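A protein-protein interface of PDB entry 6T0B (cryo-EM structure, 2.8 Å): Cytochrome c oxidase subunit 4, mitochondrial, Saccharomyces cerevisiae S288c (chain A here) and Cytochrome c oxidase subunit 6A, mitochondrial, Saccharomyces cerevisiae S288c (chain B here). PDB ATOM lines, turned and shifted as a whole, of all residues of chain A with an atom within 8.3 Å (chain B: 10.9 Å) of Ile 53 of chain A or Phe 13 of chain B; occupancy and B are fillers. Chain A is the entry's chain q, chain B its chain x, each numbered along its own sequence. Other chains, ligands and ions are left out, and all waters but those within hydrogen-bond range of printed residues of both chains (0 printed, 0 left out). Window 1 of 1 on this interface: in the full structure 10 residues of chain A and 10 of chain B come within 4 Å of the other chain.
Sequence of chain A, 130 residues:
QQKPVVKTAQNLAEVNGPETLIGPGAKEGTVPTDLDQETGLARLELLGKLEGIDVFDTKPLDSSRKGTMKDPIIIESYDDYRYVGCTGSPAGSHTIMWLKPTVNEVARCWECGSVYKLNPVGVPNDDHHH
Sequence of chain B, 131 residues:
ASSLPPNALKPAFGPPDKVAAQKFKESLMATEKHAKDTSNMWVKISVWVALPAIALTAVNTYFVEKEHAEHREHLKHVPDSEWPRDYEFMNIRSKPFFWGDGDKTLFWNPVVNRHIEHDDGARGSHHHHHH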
ATOM      1  N   LEU A  12       9.957 -21.660  10.982  1.00  0.00           N
ATOM      2  CA  LEU A  12      10.990 -21.587  12.006  1.00  0.00           C
ATOM      3  C   LEU A  12      11.464 -20.173  12.283  1.00  0.00           C
ATOM      4  O   LEU A  12      11.793 -19.858  13.429  1.00  0.00           O
ATOM      5  CB  LEU A  12      12.159 -22.483  11.608  1.00  0.00           C
ATOM      6  CG  LEU A  12      13.303 -22.699  12.585  1.00  0.00           C
ATOM      7  CD1 LEU A  12      13.735 -24.129  12.504  1.00  0.00           C
ATOM      8  CD2 LEU A  12      14.460 -21.831  12.169  1.00  0.00           C
ATOM      9  N   LEU A  44      10.422 -27.647  17.626  1.00  0.00           N
ATOM     10  CA  LEU A  44      11.549 -26.934  17.044  1.00  0.00           C
ATOM     11  C   LEU A  44      12.239 -27.785  15.996  1.00  0.00           C
ATOM     12  O   LEU A  44      12.464 -27.343  14.862  1.00  0.00           O
ATOM     13  CB  LEU A  44      12.509 -26.567  18.169  1.00  0.00           C
ATOM     14  CG  LEU A  44      13.740 -25.688  18.053  1.00  0.00           C
ATOM     15  CD1 LEU A  44      13.914 -25.013  19.376  1.00  0.00           C
ATOM     16  CD2 LEU A  44      14.946 -26.533  17.796  1.00  0.00           C
ATOM     17  N   GLU A  45      12.542 -29.028  16.364  1.00  0.00           N
ATOM     18  CA  GLU A  45      13.103 -30.012  15.452  1.00  0.00           C
ATOM     19  C   GLU A  45      12.184 -30.279  14.272  1.00  0.00           C
ATOM     20  O   GLU A  45      12.660 -30.508  13.159  1.00  0.00           O
ATOM     21  CB  GLU A  45      13.377 -31.300  16.224  1.00  0.00           C
ATOM     22  CG  GLU A  45      14.020 -32.389  15.424  1.00  0.00           C
ATOM     23  CD  GLU A  45      13.830 -33.743  16.056  1.00  0.00           C
ATOM     24  OE1 GLU A  45      12.831 -33.940  16.784  1.00  0.00           O
ATOM     25  OE2 GLU A  45      14.695 -34.608  15.837  1.00  0.00           O
ATOM     26  N   LEU A  46      10.875 -30.192  14.482  1.00  0.00           N
ATOM     27  CA  LEU A  46       9.942 -30.491  13.409  1.00  0.00           C
ATOM     28  C   LEU A  46       9.865 -29.354  12.399  1.00  0.00           C
ATOM     29  O   LEU A  46       9.837 -29.597  11.183  1.00  0.00           O
ATOM     30  CB  LEU A  46       8.585 -30.796  14.018  1.00  0.00           C
ATOM     31  CG  LEU A  46       7.544 -31.372  13.093  1.00  0.00           C
ATOM     32  CD1 LEU A  46       6.907 -32.384  13.949  1.00  0.00           C
ATOM     33  CD2 LEU A  46       6.531 -30.331  12.694  1.00  0.00           C
ATOM     34  N   LEU A  47       9.721 -28.115  12.888  1.00  0.00           N
ATOM     35  CA  LEU A  47       9.733 -26.939  12.019  1.00  0.00           C
ATOM     36  C   LEU A  47      11.032 -26.863  11.246  1.00  0.00           C
ATOM     37  O   LEU A  47      11.041 -26.521  10.053  1.00  0.00           O
ATOM     38  CB  LEU A  47       9.552 -25.672  12.842  1.00  0.00           C
ATOM     39  CG  LEU A  47       8.139 -25.483  13.350  1.00  0.00           C
ATOM     40  CD1 LEU A  47       8.097 -24.380  14.384  1.00  0.00           C
ATOM     41  CD2 LEU A  47       7.228 -25.168  12.186  1.00  0.00           C
ATOM     42  N   GLY A  48      12.130 -27.216  11.908  1.00  0.00           N
ATOM     43  CA  GLY A  48      13.357 -27.533  11.236  1.00  0.00           C
ATOM     44  C   GLY A  48      13.205 -28.564  10.146  1.00  0.00           C
ATOM     45  O   GLY A  48      13.517 -28.262   9.007  1.00  0.00           O
ATOM     46  N   LYS A  49      12.780 -29.777  10.449  1.00  0.00           N
ATOM     47  CA  LYS A  49      12.980 -30.837   9.475  1.00  0.00           C
ATOM     48  C   LYS A  49      11.994 -30.787   8.320  1.00  0.00           C
ATOM     49  O   LYS A  49      12.257 -31.420   7.290  1.00  0.00           O
ATOM     50  CB  LYS A  49      12.928 -32.207  10.148  1.00  0.00           C
ATOM     51  CG  LYS A  49      11.606 -32.548  10.757  1.00  0.00           C
ATOM     52  CD  LYS A  49      11.743 -33.773  11.639  1.00  0.00           C
ATOM     53  CE  LYS A  49      10.477 -34.024  12.437  1.00  0.00           C
ATOM     54  NZ  LYS A  49       9.306 -34.314  11.573  1.00  0.00           N
ATOM     55  N   LEU A  50      10.880 -30.054   8.451  1.00  0.00           N
ATOM     56  CA  LEU A  50      10.014 -29.868   7.286  1.00  0.00           C
ATOM     57  C   LEU A  50      10.240 -28.539   6.592  1.00  0.00           C
ATOM     58  O   LEU A  50       9.792 -28.357   5.459  1.00  0.00           O
ATOM     59  CB  LEU A  50       8.540 -30.026   7.646  1.00  0.00           C
ATOM     60  CG  LEU A  50       7.697 -29.012   8.401  1.00  0.00           C
ATOM     61  CD1 LEU A  50       7.014 -27.936   7.549  1.00  0.00           C
ATOM     62  CD2 LEU A  50       6.660 -29.841   9.054  1.00  0.00           C
ATOM     63  N   GLU A  51      10.907 -27.600   7.246  1.00  0.00           N
ATOM     64  CA  GLU A  51      11.734 -26.661   6.506  1.00  0.00           C
ATOM     65  C   GLU A  51      13.143 -27.190   6.306  1.00  0.00           C
ATOM     66  O   GLU A  51      14.087 -26.402   6.351  1.00  0.00           O
ATOM     67  CB  GLU A  51      11.781 -25.308   7.211  1.00  0.00           C
ATOM     68  CG  GLU A  51      10.617 -24.394   6.870  1.00  0.00           C
ATOM     69  CD  GLU A  51      10.922 -22.968   7.236  1.00  0.00           C
ATOM     70  OE1 GLU A  51      11.756 -22.765   8.144  1.00  0.00           O
ATOM     71  OE2 GLU A  51      10.359 -22.062   6.599  1.00  0.00           O
ATOM     72  N   GLY A  52      13.301 -28.516   6.324  1.00  0.00           N
ATOM     73  CA  GLY A  52      14.484 -29.299   6.010  1.00  0.00           C
ATOM     74  C   GLY A  52      15.746 -29.164   6.829  1.00  0.00           C
ATOM     75  O   GLY A  52      16.554 -30.093   6.885  1.00  0.00           O
ATOM     76  N   ILE A  53      15.875 -28.028   7.516  1.00  0.00           N
ATOM     77  CA  ILE A  53      17.006 -27.761   8.391  1.00  0.00           C
ATOM     78  C   ILE A  53      17.036 -28.787   9.526  1.00  0.00           C
ATOM     79  O   ILE A  53      16.016 -29.355   9.904  1.00  0.00           O
ATOM     80  CB  ILE A  53      16.855 -26.327   8.925  1.00  0.00           C
ATOM     81  CG1 ILE A  53      16.810 -25.344   7.787  1.00  0.00           C
ATOM     82  CG2 ILE A  53      17.934 -25.914   9.923  1.00  0.00           C
ATOM     83  CD1 ILE A  53      18.158 -25.046   7.175  1.00  0.00           C
ATOM     84  N   ASP A  54      18.222 -29.128   9.994  1.00  0.00           N
ATOM     85  CA  ASP A  54      18.182 -29.742  11.302  1.00  0.00           C
ATOM     86  C   ASP A  54      19.210 -29.043  12.144  1.00  0.00           C
ATOM     87  O   ASP A  54      20.406 -29.099  11.851  1.00  0.00           O
ATOM     88  CB  ASP A  54      18.405 -31.256  11.261  1.00  0.00           C
ATOM     89  CG  ASP A  54      18.009 -31.940  12.562  1.00  0.00           C
ATOM     90  OD1 ASP A  54      16.819 -31.872  12.945  1.00  0.00           O
ATOM     91  OD2 ASP A  54      18.871 -32.599  13.176  1.00  0.00           O
ATOM     92  N   VAL A  55      18.716 -28.339  13.157  1.00  0.00           N
ATOM     93  CA  VAL A  55      19.540 -28.027  14.280  1.00  0.00           C
ATOM     94  C   VAL A  55      20.080 -29.327  14.864  1.00  0.00           C
ATOM     95  O   VAL A  55      19.429 -30.379  14.826  1.00  0.00           O
ATOM     96  CB  VAL A  55      18.713 -27.239  15.299  1.00  0.00           C
ATOM     97  CG1 VAL A  55      18.401 -25.879  14.745  1.00  0.00           C
ATOM     98  CG2 VAL A  55      17.427 -27.956  15.535  1.00  0.00           C
ATOM     99  N   PHE A  56      21.287 -29.233  15.416  1.00  0.00           N
ATOM    100  CA  PHE A  56      22.191 -30.350  15.704  1.00  0.00           C
ATOM    101  C   PHE A  56      22.548 -31.081  14.424  1.00  0.00           C
ATOM    102  O   PHE A  56      22.229 -32.254  14.210  1.00  0.00           O
ATOM    103  CB  PHE A  56      21.629 -31.292  16.766  1.00  0.00           C
ATOM    104  CG  PHE A  56      21.025 -30.555  17.868  1.00  0.00           C
ATOM    105  CD1 PHE A  56      21.795 -29.636  18.520  1.00  0.00           C
ATOM    106  CD2 PHE A  56      19.686 -30.688  18.205  1.00  0.00           C
ATOM    107  CE1 PHE A  56      21.276 -28.883  19.458  1.00  0.00           C
ATOM    108  CE2 PHE A  56      19.161 -29.925  19.228  1.00  0.00           C
ATOM    109  CZ  PHE A  56      19.977 -29.017  19.863  1.00  0.00           C
ATOM    110  N   ASP A  57      23.230 -30.350  13.558  1.00  0.00           N
ATOM    111  CA  ASP A  57      23.974 -31.021  12.518  1.00  0.00           C
ATOM    112  C   ASP A  57      25.129 -31.772  13.170  1.00  0.00           C
ATOM    113  O   ASP A  57      25.696 -31.340  14.180  1.00  0.00           O
ATOM    114  CB  ASP A  57      24.433 -30.036  11.425  1.00  0.00           C
ATOM    115  CG  ASP A  57      25.240 -28.847  11.962  1.00  0.00           C
ATOM    116  OD1 ASP A  57      25.547 -28.782  13.165  1.00  0.00           O
ATOM    117  OD2 ASP A  57      25.569 -27.946  11.159  1.00  0.00           O
ATOM    118  N   TYR A  78      28.716 -22.150  20.732  1.00  0.00           N
ATOM    119  CA  TYR A  78      27.887 -21.269  21.534  1.00  0.00           C
ATOM    120  C   TYR A  78      28.427 -21.105  22.952  1.00  0.00           C
ATOM    121  O   TYR A  78      27.725 -20.568  23.816  1.00  0.00           O
ATOM    122  CB  TYR A  78      26.445 -21.784  21.545  1.00  0.00           C
ATOM    123  CG  TYR A  78      25.733 -21.602  20.217  1.00  0.00           C
ATOM    124  CD1 TYR A  78      25.942 -22.473  19.165  1.00  0.00           C
ATOM    125  CD2 TYR A  78      24.858 -20.551  20.019  1.00  0.00           C
ATOM    126  CE1 TYR A  78      25.308 -22.296  17.958  1.00  0.00           C
ATOM    127  CE2 TYR A  78      24.223 -20.366  18.818  1.00  0.00           C
ATOM    128  CZ  TYR A  78      24.450 -21.244  17.795  1.00  0.00           C
ATOM    129  OH  TYR A  78      23.818 -21.076  16.590  1.00  0.00           O
ATOM    130  N   ALA B   8      24.575 -11.365  16.862  1.00  0.00           N
ATOM    131  CA  ALA B   8      23.220 -11.629  17.320  1.00  0.00           C
ATOM    132  C   ALA B   8      22.260 -11.905  16.171  1.00  0.00           C
ATOM    133  O   ALA B   8      21.451 -12.835  16.252  1.00  0.00           O
ATOM    134  CB  ALA B   8      22.706 -10.449  18.149  1.00  0.00           C
ATOM    135  N   LEU B   9      22.341 -11.132  15.092  1.00  0.00           N
ATOM    136  CA  LEU B   9      21.330 -11.159  14.048  1.00  0.00           C
ATOM    137  C   LEU B   9      21.768 -11.898  12.795  1.00  0.00           C
ATOM    138  O   LEU B   9      21.049 -11.860  11.791  1.00  0.00           O
ATOM    139  CB  LEU B   9      20.915  -9.732  13.681  1.00  0.00           C
ATOM    140  CG  LEU B   9      20.202  -8.929  14.769  1.00  0.00           C
ATOM    141  CD1 LEU B   9      19.953  -7.500  14.312  1.00  0.00           C
ATOM    142  CD2 LEU B   9      18.899  -9.608  15.164  1.00  0.00           C
ATOM    143  N   LYS B  10      22.907 -12.566  12.818  1.00  0.00           N
ATOM    144  CA  LYS B  10      23.352 -13.271  11.629  1.00  0.00           C
ATOM    145  C   LYS B  10      22.665 -14.633  11.522  1.00  0.00           C
ATOM    146  O   LYS B  10      22.298 -15.229  12.539  1.00  0.00           O
ATOM    147  CB  LYS B  10      24.866 -13.444  11.655  1.00  0.00           C
ATOM    148  CG  LYS B  10      25.620 -12.132  11.538  1.00  0.00           C
ATOM    149  CD  LYS B  10      27.121 -12.338  11.540  1.00  0.00           C
ATOM    150  CE  LYS B  10      27.843 -11.021  11.322  1.00  0.00           C
ATOM    151  NZ  LYS B  10      27.628 -10.085  12.459  1.00  0.00           N
ATOM    152  N   PRO B  11      22.448 -15.128  10.302  1.00  0.00           N
ATOM    153  CA  PRO B  11      21.837 -16.451  10.141  1.00  0.00           C
ATOM    154  C   PRO B  11      22.757 -17.558  10.623  1.00  0.00           C
ATOM    155  O   PRO B  11      23.968 -17.386  10.763  1.00  0.00           O
ATOM    156  CB  PRO B  11      21.597 -16.553   8.633  1.00  0.00           C
ATOM    157  CG  PRO B  11      21.533 -15.140   8.168  1.00  0.00           C
ATOM    158  CD  PRO B  11      22.524 -14.409   9.019  1.00  0.00           C
ATOM    159  N   ALA B  12      22.157 -18.716  10.875  1.00  0.00           N
ATOM    160  CA  ALA B  12      22.871 -19.827  11.488  1.00  0.00           C
ATOM    161  C   ALA B  12      23.186 -20.974  10.539  1.00  0.00           C
ATOM    162  O   ALA B  12      24.226 -21.616  10.692  1.00  0.00           O
ATOM    163  CB  ALA B  12      22.072 -20.367  12.680  1.00  0.00           C
ATOM    164  N   PHE B  13      22.326 -21.259   9.558  1.00  0.00           N
ATOM    165  CA  PHE B  13      22.471 -22.467   8.751  1.00  0.00           C
ATOM    166  C   PHE B  13      22.671 -22.172   7.269  1.00  0.00           C
ATOM    167  O   PHE B  13      22.397 -23.034   6.427  1.00  0.00           O
ATOM    168  CB  PHE B  13      21.267 -23.380   8.968  1.00  0.00           C
ATOM    169  CG  PHE B  13      20.753 -23.344  10.365  1.00  0.00           C
ATOM    170  CD1 PHE B  13      21.493 -23.891  11.399  1.00  0.00           C
ATOM    171  CD2 PHE B  13      19.552 -22.723  10.656  1.00  0.00           C
ATOM    172  CE1 PHE B  13      21.032 -23.840  12.693  1.00  0.00           C
ATOM    173  CE2 PHE B  13      19.088 -22.672  11.945  1.00  0.00           C
ATOM    174  CZ  PHE B  13      19.829 -23.223  12.963  1.00  0.00           C
ATOM    175  N   GLY B  14      23.151 -20.977   6.934  1.00  0.00           N
ATOM    176  CA  GLY B  14      23.567 -20.663   5.588  1.00  0.00           C
ATOM    177  C   GLY B  14      22.416 -20.499   4.617  1.00  0.00           C
ATOM    178  O   GLY B  14      21.573 -19.608   4.769  1.00  0.00           O
ATOM    179  N   PRO B  15      22.382 -21.337   3.580  1.00  0.00           N
ATOM    180  CA  PRO B  15      21.241 -21.351   2.655  1.00  0.00           C
ATOM    181  C   PRO B  15      19.969 -21.746   3.380  1.00  0.00           C
ATOM    182  O   PRO B  15      20.025 -22.562   4.314  1.00  0.00           O
ATOM    183  CB  PRO B  15      21.640 -22.410   1.616  1.00  0.00           C
ATOM    184  CG  PRO B  15      23.125 -22.480   1.696  1.00  0.00           C
ATOM    185  CD  PRO B  15      23.460 -22.239   3.136  1.00  0.00           C
ATOM    186  N   PRO B  16      18.821 -21.157   3.007  1.00  0.00           N
ATOM    187  CA  PRO B  16      17.589 -21.366   3.794  1.00  0.00           C
ATOM    188  C   PRO B  16      17.111 -22.802   3.827  1.00  0.00           C
ATOM    189  O   PRO B  16      16.656 -23.245   4.891  1.00  0.00           O
ATOM    190  CB  PRO B  16      16.574 -20.435   3.110  1.00  0.00           C
ATOM    191  CG  PRO B  16      17.414 -19.417   2.397  1.00  0.00           C
ATOM    192  CD  PRO B  16      18.630 -20.162   1.939  1.00  0.00           C
ATOM    193  N   ASP B  17      17.242 -23.531   2.714  1.00  0.00           N
ATOM    194  CA  ASP B  17      16.981 -24.960   2.687  1.00  0.00           C
ATOM    195  C   ASP B  17      17.444 -25.606   1.391  1.00  0.00           C
ATOM    196  O   ASP B  17      17.649 -24.960   0.361  1.00  0.00           O
ATOM    197  CB  ASP B  17      15.507 -25.316   2.866  1.00  0.00           C
ATOM    198  CG  ASP B  17      15.345 -26.571   3.668  1.00  0.00           C
ATOM    199  OD1 ASP B  17      16.203 -26.822   4.557  1.00  0.00           O
ATOM    200  OD2 ASP B  17      14.360 -27.295   3.475  1.00  0.00           O
ATOM    201  N   LYS B  18      17.525 -26.928   1.489  1.00  0.00           N
ATOM    202  CA  LYS B  18      17.632 -28.008   0.514  1.00  0.00           C
ATOM    203  C   LYS B  18      16.406 -28.211  -0.370  1.00  0.00           C
ATOM    204  O   LYS B  18      15.430 -27.458  -0.289  1.00  0.00           O
ATOM    205  CB  LYS B  18      17.833 -29.295   1.303  1.00  0.00           C
ATOM    206  CG  LYS B  18      16.746 -29.369   2.349  1.00  0.00           C
ATOM    207  CD  LYS B  18      16.807 -30.490   3.336  1.00  0.00           C
ATOM    208  CE  LYS B  18      18.070 -30.429   4.093  1.00  0.00           C
ATOM    209  NZ  LYS B  18      18.251 -29.102   4.780  1.00  0.00           N
ATOM    210  N   VAL B  19      16.458 -29.252  -1.209  1.00  0.00           N
ATOM    211  CA  VAL B  19      15.282 -29.793  -1.868  1.00  0.00           C
ATOM    212  C   VAL B  19      14.609 -30.847  -0.983  1.00  0.00           C
ATOM    213  O   VAL B  19      13.437 -31.184  -1.201  1.00  0.00           O
ATOM    214  CB  VAL B  19      15.768 -30.265  -3.273  1.00  0.00           C
ATOM    215  CG1 VAL B  19      14.729 -31.054  -4.070  1.00  0.00           C
ATOM    216  CG2 VAL B  19      16.224 -29.063  -4.112  1.00  0.00           C
ATOM    217  N   ALA B  20      15.259 -31.283   0.101  1.00  0.00           N
ATOM    218  CA  ALA B  20      14.741 -32.497   0.745  1.00  0.00           C
ATOM    219  C   ALA B  20      13.654 -32.247   1.784  1.00  0.00           C
ATOM    220  O   ALA B  20      13.203 -33.211   2.411  1.00  0.00           O
ATOM    221  CB  ALA B  20      15.851 -33.362   1.364  1.00  0.00           C
ATOM    222  N   ALA B  21      13.171 -31.014   1.914  1.00  0.00           N
ATOM    223  CA  ALA B  21      11.993 -30.759   2.733  1.00  0.00           C
ATOM    224  C   ALA B  21      10.753 -31.453   2.176  1.00  0.00           C
ATOM    225  O   ALA B  21       9.940 -32.007   2.928  1.00  0.00           O
ATOM    226  CB  ALA B  21      11.756 -29.254   2.823  1.00  0.00           C
ATOM    227  N   GLN B  22      10.631 -31.504   0.854  1.00  0.00           N
ATOM    228  CA  GLN B  22       9.427 -32.041   0.222  1.00  0.00           C
ATOM    229  C   GLN B  22       9.528 -33.540  -0.011  1.00  0.00           C
ATOM    230  O   GLN B  22       8.515 -34.258   0.056  1.00  0.00           O
ATOM    231  CB  GLN B  22       9.152 -31.298  -1.090  1.00  0.00           C
ATOM    232  CG  GLN B  22       8.843 -29.798  -0.912  1.00  0.00           C
ATOM    233  CD  GLN B  22      10.064 -28.912  -0.724  1.00  0.00           C
ATOM    234  OE1 GLN B  22      11.204 -29.379  -0.752  1.00  0.00           O
ATOM    235  NE2 GLN B  22       9.825 -27.626  -0.511  1.00  0.00           N
ATOM    236  N   PHE B  24      10.911 -35.048   2.420  1.00  0.00           N
ATOM    237  CA  PHE B  24      10.442 -35.405   3.757  1.00  0.00           C
ATOM    238  C   PHE B  24       8.921 -35.359   3.885  1.00  0.00           C
ATOM    239  O   PHE B  24       8.331 -36.184   4.593  1.00  0.00           O
ATOM    240  CB  PHE B  24      11.075 -34.461   4.778  1.00  0.00           C
ATOM    241  CG  PHE B  24      10.838 -34.864   6.192  1.00  0.00           C
ATOM    242  CD1 PHE B  24      11.613 -35.854   6.762  1.00  0.00           C
ATOM    243  CD2 PHE B  24       9.835 -34.275   6.943  1.00  0.00           C
ATOM    244  CE1 PHE B  24      11.400 -36.253   8.052  1.00  0.00           C
ATOM    245  CE2 PHE B  24       9.610 -34.671   8.238  1.00  0.00           C
ATOM    246  CZ  PHE B  24      10.396 -35.662   8.794  1.00  0.00           C
ATOM    247  N   LYS B  25       8.260 -34.377   3.278  1.00  0.00           N
ATOM    248  CA  LYS B  25       6.833 -34.315   3.581  1.00  0.00           C
ATOM    249  C   LYS B  25       5.992 -35.302   2.771  1.00  0.00           C
ATOM    250  O   LYS B  25       4.968 -35.799   3.269  1.00  0.00           O
ATOM    251  CB  LYS B  25       6.321 -32.890   3.468  1.00  0.00           C
ATOM    252  CG  LYS B  25       6.811 -32.074   4.657  1.00  0.00           C
ATOM    253  CD  LYS B  25       6.117 -30.757   4.861  1.00  0.00           C
ATOM    254  CE  LYS B  25       4.692 -30.954   5.409  1.00  0.00           C
ATOM    255  NZ  LYS B  25       4.697 -31.482   6.805  1.00  0.00           N
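NZ of Lys 18 of chain B is in hydrogen-bond range of O of Gly 52 of chain A (2.9 Å). The backbone NH (N) of Ile 53 of chain A is in hydrogen-bond range of the side-chain carboxylate (OD1) of Asp 17 of chain B. N of Gly 52 of chain A lies close to OD2 of Asp 17 of chain B (3.3 Å). O of Glu 51 of chain A lies close to OD1 of Asp 17 of chain B (2.8 Å).
OD1 of Asp 17 of chain B is in salt-bridge range of NZ of Lys 18 of chain B (3.1 Å). The backbone NH (N) of Ile 53 of chain A lies within hydrogen-bond range of the backbone carbonyl oxygen (O) of Gly 48 of chain A (2.8 Å).
Lys 49 of chain A touches Phe 24 of chain B (NZ to CZ, 3.3 Å). Ala 21 of chain B touches Leu 50 of chain A (CB to O, 3.4 Å). Leu 50 of chain A touches Lys 25 of chain B. Gly 52 of chain A touches Ala 21 of chain B (N to CB, 3.9 Å). Phe 13 of chain B touches Ile 53 of chain A. Pro 16 of chain B touches Ile 53 of chain A (O to CD1, 3.3 Å). NZ of Lys 18 of chain B touches N of Ile 53 of chain A, 3.8 Å away. Val 55 of chain A touches Phe 13 of chain B.
No residue of chain B comes within 4 Å of Gly 48 of chain A. Printed residues of chain B within 4 Å of Leu 50 of chain A: Ala 21 (3.4 Å) and Lys 25 (3.4 Å). Of chain B, only Phe 13 (3.7 Å), Pro 16 (3.3 Å), Asp 17 (3.2 Å) and Lys 18 (3.8 Å) come within 4 Å of Ile 53 of chain A. No residue of chain B comes within 4 Å of Asp 54 of chain A. No residue of chain A comes within 4 Å of Ala 12 of chain B. Of chain A, only Ile 53 and Val 55 come within 4 Å of Phe 13 of chain B. Of the printed residues of chain A, Ala 21 of chain B touches Leu 50 (3.4 Å) and Gly 52 (3.9 Å). The nearest residue of chain A that does not touch Phe 13 of chain B is Leu 12 of chain A (4.7 Å).
Hydrophobic or aromatic side chains of chain A within 4 Å of the printed part of chain B: Leu 50, Ile 53 and Val 55. Among the printed residues, 12 pairs touch across the chains.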
